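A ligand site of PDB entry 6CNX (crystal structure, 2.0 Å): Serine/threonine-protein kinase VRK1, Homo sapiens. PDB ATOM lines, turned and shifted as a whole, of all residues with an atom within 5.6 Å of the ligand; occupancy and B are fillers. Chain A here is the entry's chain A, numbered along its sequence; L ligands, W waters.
Water W1 lies within hydrogen-bond range of an oxygen (O2) of the ligand (2.4 Å), the side-chain hydroxyl (OH) of Tyr 87 (2.5 Å), the side-chain carboxylate (OE2) of Glu 83 (2.6 Å) and the backbone NH (N) of Asp 197 (3.1 Å).
Water W4 lies within hydrogen-bond range of OE2 of Glu 83 (2.6 Å), NZ of Lys 71 (2.7 Å) and O2 of the ligand (2.9 Å).
Water W5 lies within hydrogen-bond range of the side-chain carboxylate of Asp 137 (2.6 Å) and an oxygen (O1) of the ligand (3.2 Å).
OH of Tyr 87 lies close to F1 of the ligand, 3.4 Å away.
Residues that only touch the ligand: Ile 43 (3.4 Å), Phe 48 (3.5 Å), Ile 51 (3.5 Å), Val 69 (3.6 Å), Glu 83 (3.6 Å), Pro 111 (3.5 Å), Met 131 (3.5 Å), Arg 133 (3.5 Å), Gly 135 (3.3 Å), Asp 137 (3.9 Å), Leu 184 (3.6 Å) and Val 196 (3.3 Å).
Of the 22 residues printed, 16 come within 4 Å of the ligand.
NZ of Lys 71 is in hydrogen-bond range of O2 of the ligand, 2.7 Å away.
The backbone NH of Phe 134 lies within hydrogen-bond range of a nitrogen (N1) of the ligand (2.8 Å).
The backbone carbonyl oxygen (O) of Asp 132 lies within hydrogen-bond range of a nitrogen (N5) of the ligand, 3.1 Å away.
NZ of Lys 71 lies within salt-bridge range of OE1 of Glu 83, at 2.7 Å.
N of Val 196 lies within hydrogen-bond range of O of Asn 182 (2.9 Å).
N of Ile 43 sits at hydrogen-bond distance from O of Ile 51 (3.0 Å).
The backbone carbonyl oxygen (O) of Met 131 sits at hydrogen-bond distance from the backbone NH (N) of Val 69, 2.8 Å away.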
ATOM      1  N   ILE A  43      15.366  24.912  25.416  1.00  0.00           N
ATOM      2  CA  ILE A  43      14.136  24.398  26.016  1.00  0.00           C
ATOM      3  C   ILE A  43      14.271  24.166  27.547  1.00  0.00           C
ATOM      4  O   ILE A  43      15.404  23.945  28.041  1.00  0.00           O
ATOM      5  CB  ILE A  43      13.596  23.106  25.365  1.00  0.00           C
ATOM      6  CG1 ILE A  43      14.606  21.962  25.366  1.00  0.00           C
ATOM      7  CG2 ILE A  43      13.166  23.378  23.939  1.00  0.00           C
ATOM      8  CD1 ILE A  43      13.934  20.595  25.239  1.00  0.00           C
ATOM      9  N   GLY A  44      13.114  24.209  28.236  1.00  0.00           N
ATOM     10  CA  GLY A  44      12.979  23.774  29.611  1.00  0.00           C
ATOM     11  C   GLY A  44      13.981  24.351  30.596  1.00  0.00           C
ATOM     12  O   GLY A  44      14.519  23.617  31.442  1.00  0.00           O
ATOM     13  N   PHE A  48      17.731  20.436  29.866  1.00  0.00           N
ATOM     14  CA  PHE A  48      17.954  19.271  28.973  1.00  0.00           C
ATOM     15  C   PHE A  48      19.145  19.498  28.019  1.00  0.00           C
ATOM     16  O   PHE A  48      19.103  19.063  26.859  1.00  0.00           O
ATOM     17  CB  PHE A  48      16.672  18.929  28.185  1.00  0.00           C
ATOM     18  CG  PHE A  48      15.475  18.635  29.056  1.00  0.00           C
ATOM     19  CD1 PHE A  48      15.268  17.338  29.582  1.00  0.00           C
ATOM     20  CD2 PHE A  48      14.535  19.659  29.356  1.00  0.00           C
ATOM     21  CE1 PHE A  48      14.163  17.074  30.396  1.00  0.00           C
ATOM     22  CE2 PHE A  48      13.417  19.389  30.171  1.00  0.00           C
ATOM     23  CZ  PHE A  48      13.244  18.102  30.689  1.00  0.00           C
ATOM     24  N   ILE A  51      19.610  21.870  23.490  1.00  0.00           N
ATOM     25  CA  ILE A  51      18.476  21.631  22.632  1.00  0.00           C
ATOM     26  C   ILE A  51      17.700  22.941  22.621  1.00  0.00           C
ATOM     27  O   ILE A  51      17.336  23.458  23.664  1.00  0.00           O
ATOM     28  CB  ILE A  51      17.583  20.507  23.175  1.00  0.00           C
ATOM     29  CG1 ILE A  51      18.342  19.178  23.245  1.00  0.00           C
ATOM     30  CG2 ILE A  51      16.331  20.365  22.321  1.00  0.00           C
ATOM     31  CD1 ILE A  51      17.560  18.078  23.926  1.00  0.00           C
ATOM     32  N   LEU A  53      14.573  25.435  20.557  1.00  0.00           N
ATOM     33  CA  LEU A  53      13.387  25.492  19.698  1.00  0.00           C
ATOM     34  C   LEU A  53      13.866  25.879  18.282  1.00  0.00           C
ATOM     35  O   LEU A  53      14.896  26.583  18.110  1.00  0.00           O
ATOM     36  CB  LEU A  53      12.418  26.531  20.203  1.00  0.00           C
ATOM     37  CG  LEU A  53      11.824  26.295  21.606  1.00  0.00           C
ATOM     38  CD1 LEU A  53      11.240  27.559  22.194  1.00  0.00           C
ATOM     39  CD2 LEU A  53      10.805  25.200  21.588  1.00  0.00           C
ATOM     40  N   VAL A  69      12.709  21.106  17.287  1.00  0.00           N
ATOM     41  CA  VAL A  69      13.882  21.442  18.054  1.00  0.00           C
ATOM     42  C   VAL A  69      15.130  21.163  17.249  1.00  0.00           C
ATOM     43  O   VAL A  69      15.123  20.360  16.309  1.00  0.00           O
ATOM     44  CB  VAL A  69      13.986  20.677  19.378  1.00  0.00           C
ATOM     45  CG1 VAL A  69      12.810  20.989  20.291  1.00  0.00           C
ATOM     46  CG2 VAL A  69      14.059  19.165  19.162  1.00  0.00           C
ATOM     47  N   LYS A  71      18.981  19.898  18.125  1.00  0.00           N
ATOM     48  CA  LYS A  71      19.986  19.350  19.028  1.00  0.00           C
ATOM     49  C   LYS A  71      21.367  19.626  18.454  1.00  0.00           C
ATOM     50  O   LYS A  71      21.598  19.384  17.261  1.00  0.00           O
ATOM     51  CB  LYS A  71      19.806  17.838  19.183  1.00  0.00           C
ATOM     52  CG  LYS A  71      18.433  17.427  19.724  1.00  0.00           C
ATOM     53  CD  LYS A  71      17.760  16.221  19.035  1.00  0.00           C
ATOM     54  CE  LYS A  71      18.550  14.926  19.103  1.00  0.00           C
ATOM     55  NZ  LYS A  71      18.465  14.273  20.446  1.00  0.00           N
ATOM     56  N   GLU A  83      22.729   8.441  17.308  1.00  0.00           N
ATOM     57  CA  GLU A  83      21.344   8.824  17.206  1.00  0.00           C
ATOM     58  C   GLU A  83      20.983   9.241  15.762  1.00  0.00           C
ATOM     59  O   GLU A  83      19.962   8.794  15.214  1.00  0.00           O
ATOM     60  CB  GLU A  83      21.069   9.921  18.217  1.00  0.00           C
ATOM     61  CG  GLU A  83      19.635  10.392  18.237  1.00  0.00           C
ATOM     62  CD  GLU A  83      19.289  11.123  19.527  1.00  0.00           C
ATOM     63  OE1 GLU A  83      19.998  12.122  19.820  1.00  0.00           O
ATOM     64  OE2 GLU A  83      18.324  10.653  20.238  1.00  0.00           O
ATOM     65  N   TYR A  87      18.167   7.493  13.154  1.00  0.00           N
ATOM     66  CA  TYR A  87      17.086   8.218  12.473  1.00  0.00           C
ATOM     67  C   TYR A  87      17.188   8.161  10.934  1.00  0.00           C
ATOM     68  O   TYR A  87      16.193   7.916  10.272  1.00  0.00           O
ATOM     69  CB  TYR A  87      17.012   9.627  13.006  1.00  0.00           C
ATOM     70  CG  TYR A  87      16.328   9.752  14.340  1.00  0.00           C
ATOM     71  CD1 TYR A  87      14.963   9.480  14.481  1.00  0.00           C
ATOM     72  CD2 TYR A  87      17.024  10.200  15.457  1.00  0.00           C
ATOM     73  CE1 TYR A  87      14.348   9.580  15.741  1.00  0.00           C
ATOM     74  CE2 TYR A  87      16.402  10.376  16.696  1.00  0.00           C
ATOM     75  CZ  TYR A  87      15.047  10.033  16.822  1.00  0.00           C
ATOM     76  OH  TYR A  87      14.384  10.201  17.995  1.00  0.00           O
ATOM     77  N   PRO A 111       9.979   9.416  16.810  1.00  0.00           N
ATOM     78  CA  PRO A 111      10.070  10.835  16.460  1.00  0.00           C
ATOM     79  C   PRO A 111      10.485  11.058  15.021  1.00  0.00           C
ATOM     80  O   PRO A 111      11.266  10.312  14.467  1.00  0.00           O
ATOM     81  CB  PRO A 111      11.140  11.350  17.423  1.00  0.00           C
ATOM     82  CG  PRO A 111      11.043  10.435  18.586  1.00  0.00           C
ATOM     83  CD  PRO A 111      10.788   9.090  17.995  1.00  0.00           C
ATOM     84  N   MET A 131      14.584  17.861  14.884  1.00  0.00           N
ATOM     85  CA  MET A 131      13.572  16.877  15.214  1.00  0.00           C
ATOM     86  C   MET A 131      12.281  17.541  15.620  1.00  0.00           C
ATOM     87  O   MET A 131      12.204  18.738  15.810  1.00  0.00           O
ATOM     88  CB  MET A 131      14.004  16.055  16.433  1.00  0.00           C
ATOM     89  CG  MET A 131      15.421  15.538  16.401  1.00  0.00           C
ATOM     90  SD  MET A 131      15.559  14.221  15.204  1.00  0.00           S
ATOM     91  CE  MET A 131      14.228  13.144  15.711  1.00  0.00           C
ATOM     92  N   ASP A 132      11.271  16.719  15.791  1.00  0.00           N
ATOM     93  CA  ASP A 132      10.000  17.194  16.263  1.00  0.00           C
ATOM     94  C   ASP A 132      10.079  17.724  17.667  1.00  0.00           C
ATOM     95  O   ASP A 132      10.783  17.195  18.495  1.00  0.00           O
ATOM     96  CB  ASP A 132       9.056  16.017  16.362  1.00  0.00           C
ATOM     97  CG  ASP A 132       8.341  15.757  15.100  1.00  0.00           C
ATOM     98  OD1 ASP A 132       8.268  16.672  14.270  1.00  0.00           O
ATOM     99  OD2 ASP A 132       7.898  14.612  14.952  1.00  0.00           O
ATOM    100  N   ARG A 133       9.354  18.800  17.910  1.00  0.00           N
ATOM    101  CA  ARG A 133       9.162  19.306  19.247  1.00  0.00           C
ATOM    102  C   ARG A 133       7.941  18.556  19.873  1.00  0.00           C
ATOM    103  O   ARG A 133       6.874  18.447  19.258  1.00  0.00           O
ATOM    104  CB  ARG A 133       8.875  20.810  19.226  1.00  0.00           C
ATOM    105  CG  ARG A 133       8.669  21.430  20.596  1.00  0.00           C
ATOM    106  CD  ARG A 133       7.220  21.488  21.007  1.00  0.00           C
ATOM    107  NE  ARG A 133       7.021  22.189  22.277  1.00  0.00           N
ATOM    108  CZ  ARG A 133       6.993  23.517  22.421  1.00  0.00           C
ATOM    109  NH1 ARG A 133       6.833  24.003  23.639  1.00  0.00           N
ATOM    110  NH2 ARG A 133       7.098  24.341  21.385  1.00  0.00           N
ATOM    111  N   PHE A 134       8.130  18.098  21.103  1.00  0.00           N
ATOM    112  CA  PHE A 134       7.063  17.449  21.889  1.00  0.00           C
ATOM    113  C   PHE A 134       6.584  18.303  23.089  1.00  0.00           C
ATOM    114  O   PHE A 134       7.103  19.397  23.363  1.00  0.00           O
ATOM    115  CB  PHE A 134       7.612  16.087  22.377  1.00  0.00           C
ATOM    116  CG  PHE A 134       7.889  15.141  21.251  1.00  0.00           C
ATOM    117  CD1 PHE A 134       6.850  14.576  20.538  1.00  0.00           C
ATOM    118  CD2 PHE A 134       9.179  14.853  20.878  1.00  0.00           C
ATOM    119  CE1 PHE A 134       7.085  13.666  19.508  1.00  0.00           C
ATOM    120  CE2 PHE A 134       9.431  13.940  19.838  1.00  0.00           C
ATOM    121  CZ  PHE A 134       8.348  13.357  19.157  1.00  0.00           C
ATOM    122  N   GLY A 135       5.566  17.791  23.767  1.00  0.00           N
ATOM    123  CA  GLY A 135       5.136  18.353  25.039  1.00  0.00           C
ATOM    124  C   GLY A 135       5.891  17.695  26.182  1.00  0.00           C
ATOM    125  O   GLY A 135       7.112  17.421  26.107  1.00  0.00           O
ATOM    126  N   SER A 136       5.170  17.400  27.235  1.00  0.00           N
ATOM    127  CA  SER A 136       5.789  16.956  28.484  1.00  0.00           C
ATOM    128  C   SER A 136       6.293  15.518  28.367  1.00  0.00           C
ATOM    129  O   SER A 136       5.752  14.690  27.615  1.00  0.00           O
ATOM    130  CB  SER A 136       4.757  17.044  29.605  1.00  0.00           C
ATOM    131  OG  SER A 136       5.302  16.536  30.815  1.00  0.00           O
ATOM    132  N   ASP A 137       7.348  15.229  29.134  1.00  0.00           N
ATOM    133  CA  ASP A 137       7.741  13.837  29.370  1.00  0.00           C
ATOM    134  C   ASP A 137       6.766  13.196  30.368  1.00  0.00           C
ATOM    135  O   ASP A 137       6.089  13.894  31.115  1.00  0.00           O
ATOM    136  CB  ASP A 137       9.201  13.732  29.831  1.00  0.00           C
ATOM    137  CG  ASP A 137       9.430  14.292  31.217  1.00  0.00           C
ATOM    138  OD1 ASP A 137       9.205  13.638  32.204  1.00  0.00           O
ATOM    139  OD2 ASP A 137       9.850  15.428  31.330  1.00  0.00           O
ATOM    140  N   SER A 181      10.958   9.181  31.635  1.00  0.00           N
ATOM    141  CA  SER A 181      11.645  10.403  31.186  1.00  0.00           C
ATOM    142  C   SER A 181      12.057  10.383  29.694  1.00  0.00           C
ATOM    143  O   SER A 181      12.351  11.449  29.123  1.00  0.00           O
ATOM    144  CB  SER A 181      12.864  10.746  32.067  1.00  0.00           C
ATOM    145  OG  SER A 181      13.852   9.764  31.931  1.00  0.00           O
ATOM    146  N   ASN A 182      12.084   9.184  29.083  1.00  0.00           N
ATOM    147  CA  ASN A 182      12.312   9.033  27.630  1.00  0.00           C
ATOM    148  C   ASN A 182      11.013   8.832  26.819  1.00  0.00           C
ATOM    149  O   ASN A 182      11.060   8.454  25.649  1.00  0.00           O
ATOM    150  CB  ASN A 182      13.293   7.884  27.367  1.00  0.00           C
ATOM    151  CG  ASN A 182      14.751   8.272  27.696  1.00  0.00           C
ATOM    152  OD1 ASN A 182      15.100   9.449  27.673  1.00  0.00           O
ATOM    153  ND2 ASN A 182      15.593   7.289  28.052  1.00  0.00           N
ATOM    154  N   LEU A 184       7.660  10.939  25.620  1.00  0.00           N
ATOM    155  CA  LEU A 184       7.150  12.307  25.456  1.00  0.00           C
ATOM    156  C   LEU A 184       5.843  12.296  24.718  1.00  0.00           C
ATOM    157  O   LEU A 184       5.644  11.486  23.817  1.00  0.00           O
ATOM    158  CB  LEU A 184       8.119  13.223  24.681  1.00  0.00           C
ATOM    159  CG  LEU A 184       9.587  13.306  25.024  1.00  0.00           C
ATOM    160  CD1 LEU A 184      10.379  14.340  24.267  1.00  0.00           C
ATOM    161  CD2 LEU A 184       9.855  13.419  26.507  1.00  0.00           C
ATOM    162  N   VAL A 196      11.913   8.522  22.872  1.00  0.00           N
ATOM    163  CA  VAL A 196      13.033   9.335  22.451  1.00  0.00           C
ATOM    164  C   VAL A 196      14.339   8.852  23.076  1.00  0.00           C
ATOM    165  O   VAL A 196      14.334   7.909  23.867  1.00  0.00           O
ATOM    166  CB  VAL A 196      12.803  10.828  22.748  1.00  0.00           C
ATOM    167  CG1 VAL A 196      11.480  11.291  22.182  1.00  0.00           C
ATOM    168  CG2 VAL A 196      12.859  11.082  24.241  1.00  0.00           C
ATOM    169  N   ASP A 197      15.445   9.443  22.597  1.00  0.00           N
ATOM    170  CA  ASP A 197      16.821   9.184  23.037  1.00  0.00           C
ATOM    171  C   ASP A 197      17.428   7.909  22.471  1.00  0.00           C
ATOM    172  O   ASP A 197      17.310   6.857  23.053  1.00  0.00           O
ATOM    173  CB  ASP A 197      17.075   9.379  24.544  1.00  0.00           C
ATOM    174  CG  ASP A 197      18.531   9.469  24.884  1.00  0.00           C
ATOM    175  OD1 ASP A 197      19.377   9.059  24.071  1.00  0.00           O
ATOM    176  OD2 ASP A 197      18.830   9.951  25.978  1.00  0.00           O
HETATM  177  N1  LIG L   1      10.520  18.449  22.494  1.00  0.00           N
HETATM  178  C1  LIG L   1      10.693  18.716  24.854  1.00  0.00           C
HETATM  179  C2  LIG L   1      11.812  17.873  24.825  1.00  0.00           C
HETATM  180  C3  LIG L   1      10.829  18.986  27.271  1.00  0.00           C
HETATM  181  C4  LIG L   1      11.910  17.926  27.300  1.00  0.00           C
HETATM  182  C5  LIG L   1       9.051  20.130  26.058  1.00  0.00           C
HETATM  183  C6  LIG L   1       9.359  21.463  25.528  1.00  0.00           C
HETATM  184  C7  LIG L   1       9.616  22.514  25.080  1.00  0.00           C
HETATM  185  C8  LIG L   1      13.816  16.929  25.963  1.00  0.00           C
HETATM  186  C9  LIG L   1      13.804  15.418  25.863  1.00  0.00           C
HETATM  187  C10 LIG L   1      15.138  14.859  25.370  1.00  0.00           C
HETATM  188  C11 LIG L   1      11.448  16.705  28.068  1.00  0.00           C
HETATM  189  C12 LIG L   1      13.032  16.164  21.154  1.00  0.00           C
HETATM  190  C13 LIG L   1      14.248  16.220  21.821  1.00  0.00           C
HETATM  191  C14 LIG L   1      15.193  15.259  21.563  1.00  0.00           C
HETATM  192  C15 LIG L   1      14.964  14.241  20.671  1.00  0.00           C
HETATM  193  C16 LIG L   1      13.753  14.220  20.001  1.00  0.00           C
HETATM  194  C17 LIG L   1      12.787  15.173  20.223  1.00  0.00           C
HETATM  195  N2  LIG L   1      12.262  17.355  23.667  1.00  0.00           N
HETATM  196  C18 LIG L   1      11.608  17.668  22.548  1.00  0.00           C
HETATM  197  C19 LIG L   1      10.068  18.968  23.628  1.00  0.00           C
HETATM  198  N3  LIG L   1      10.220  19.257  26.064  1.00  0.00           N
HETATM  199  N4  LIG L   1      12.484  17.579  25.987  1.00  0.00           N
HETATM  200  O1  LIG L   1      10.501  19.554  28.295  1.00  0.00           O
HETATM  201  C20 LIG L   1      16.266  15.071  26.367  1.00  0.00           C
HETATM  202  C21 LIG L   1      15.053  13.395  24.971  1.00  0.00           C
HETATM  203  N5  LIG L   1      12.025  17.136  21.381  1.00  0.00           N
HETATM  204  F1  LIG L   1      13.510  13.246  19.108  1.00  0.00           F
HETATM  205  F2  LIG L   1      16.363  15.294  22.222  1.00  0.00           F
HETATM  206  O2  LIG L   1      15.911  13.311  20.447  1.00  0.00           O
HETATM  207  O   HOH W   1      15.723  10.952  19.956  1.00  0.00           O
HETATM  208  O   HOH W   2       5.977  21.783  25.859  1.00  0.00           O
HETATM  209  O   HOH W   3      12.920  14.067  29.736  1.00  0.00           O
HETATM  210  O   HOH W   4      17.939  12.305  22.247  1.00  0.00           O
HETATM  211  O   HOH W   5       8.888  17.603  30.256  1.00  0.00           O
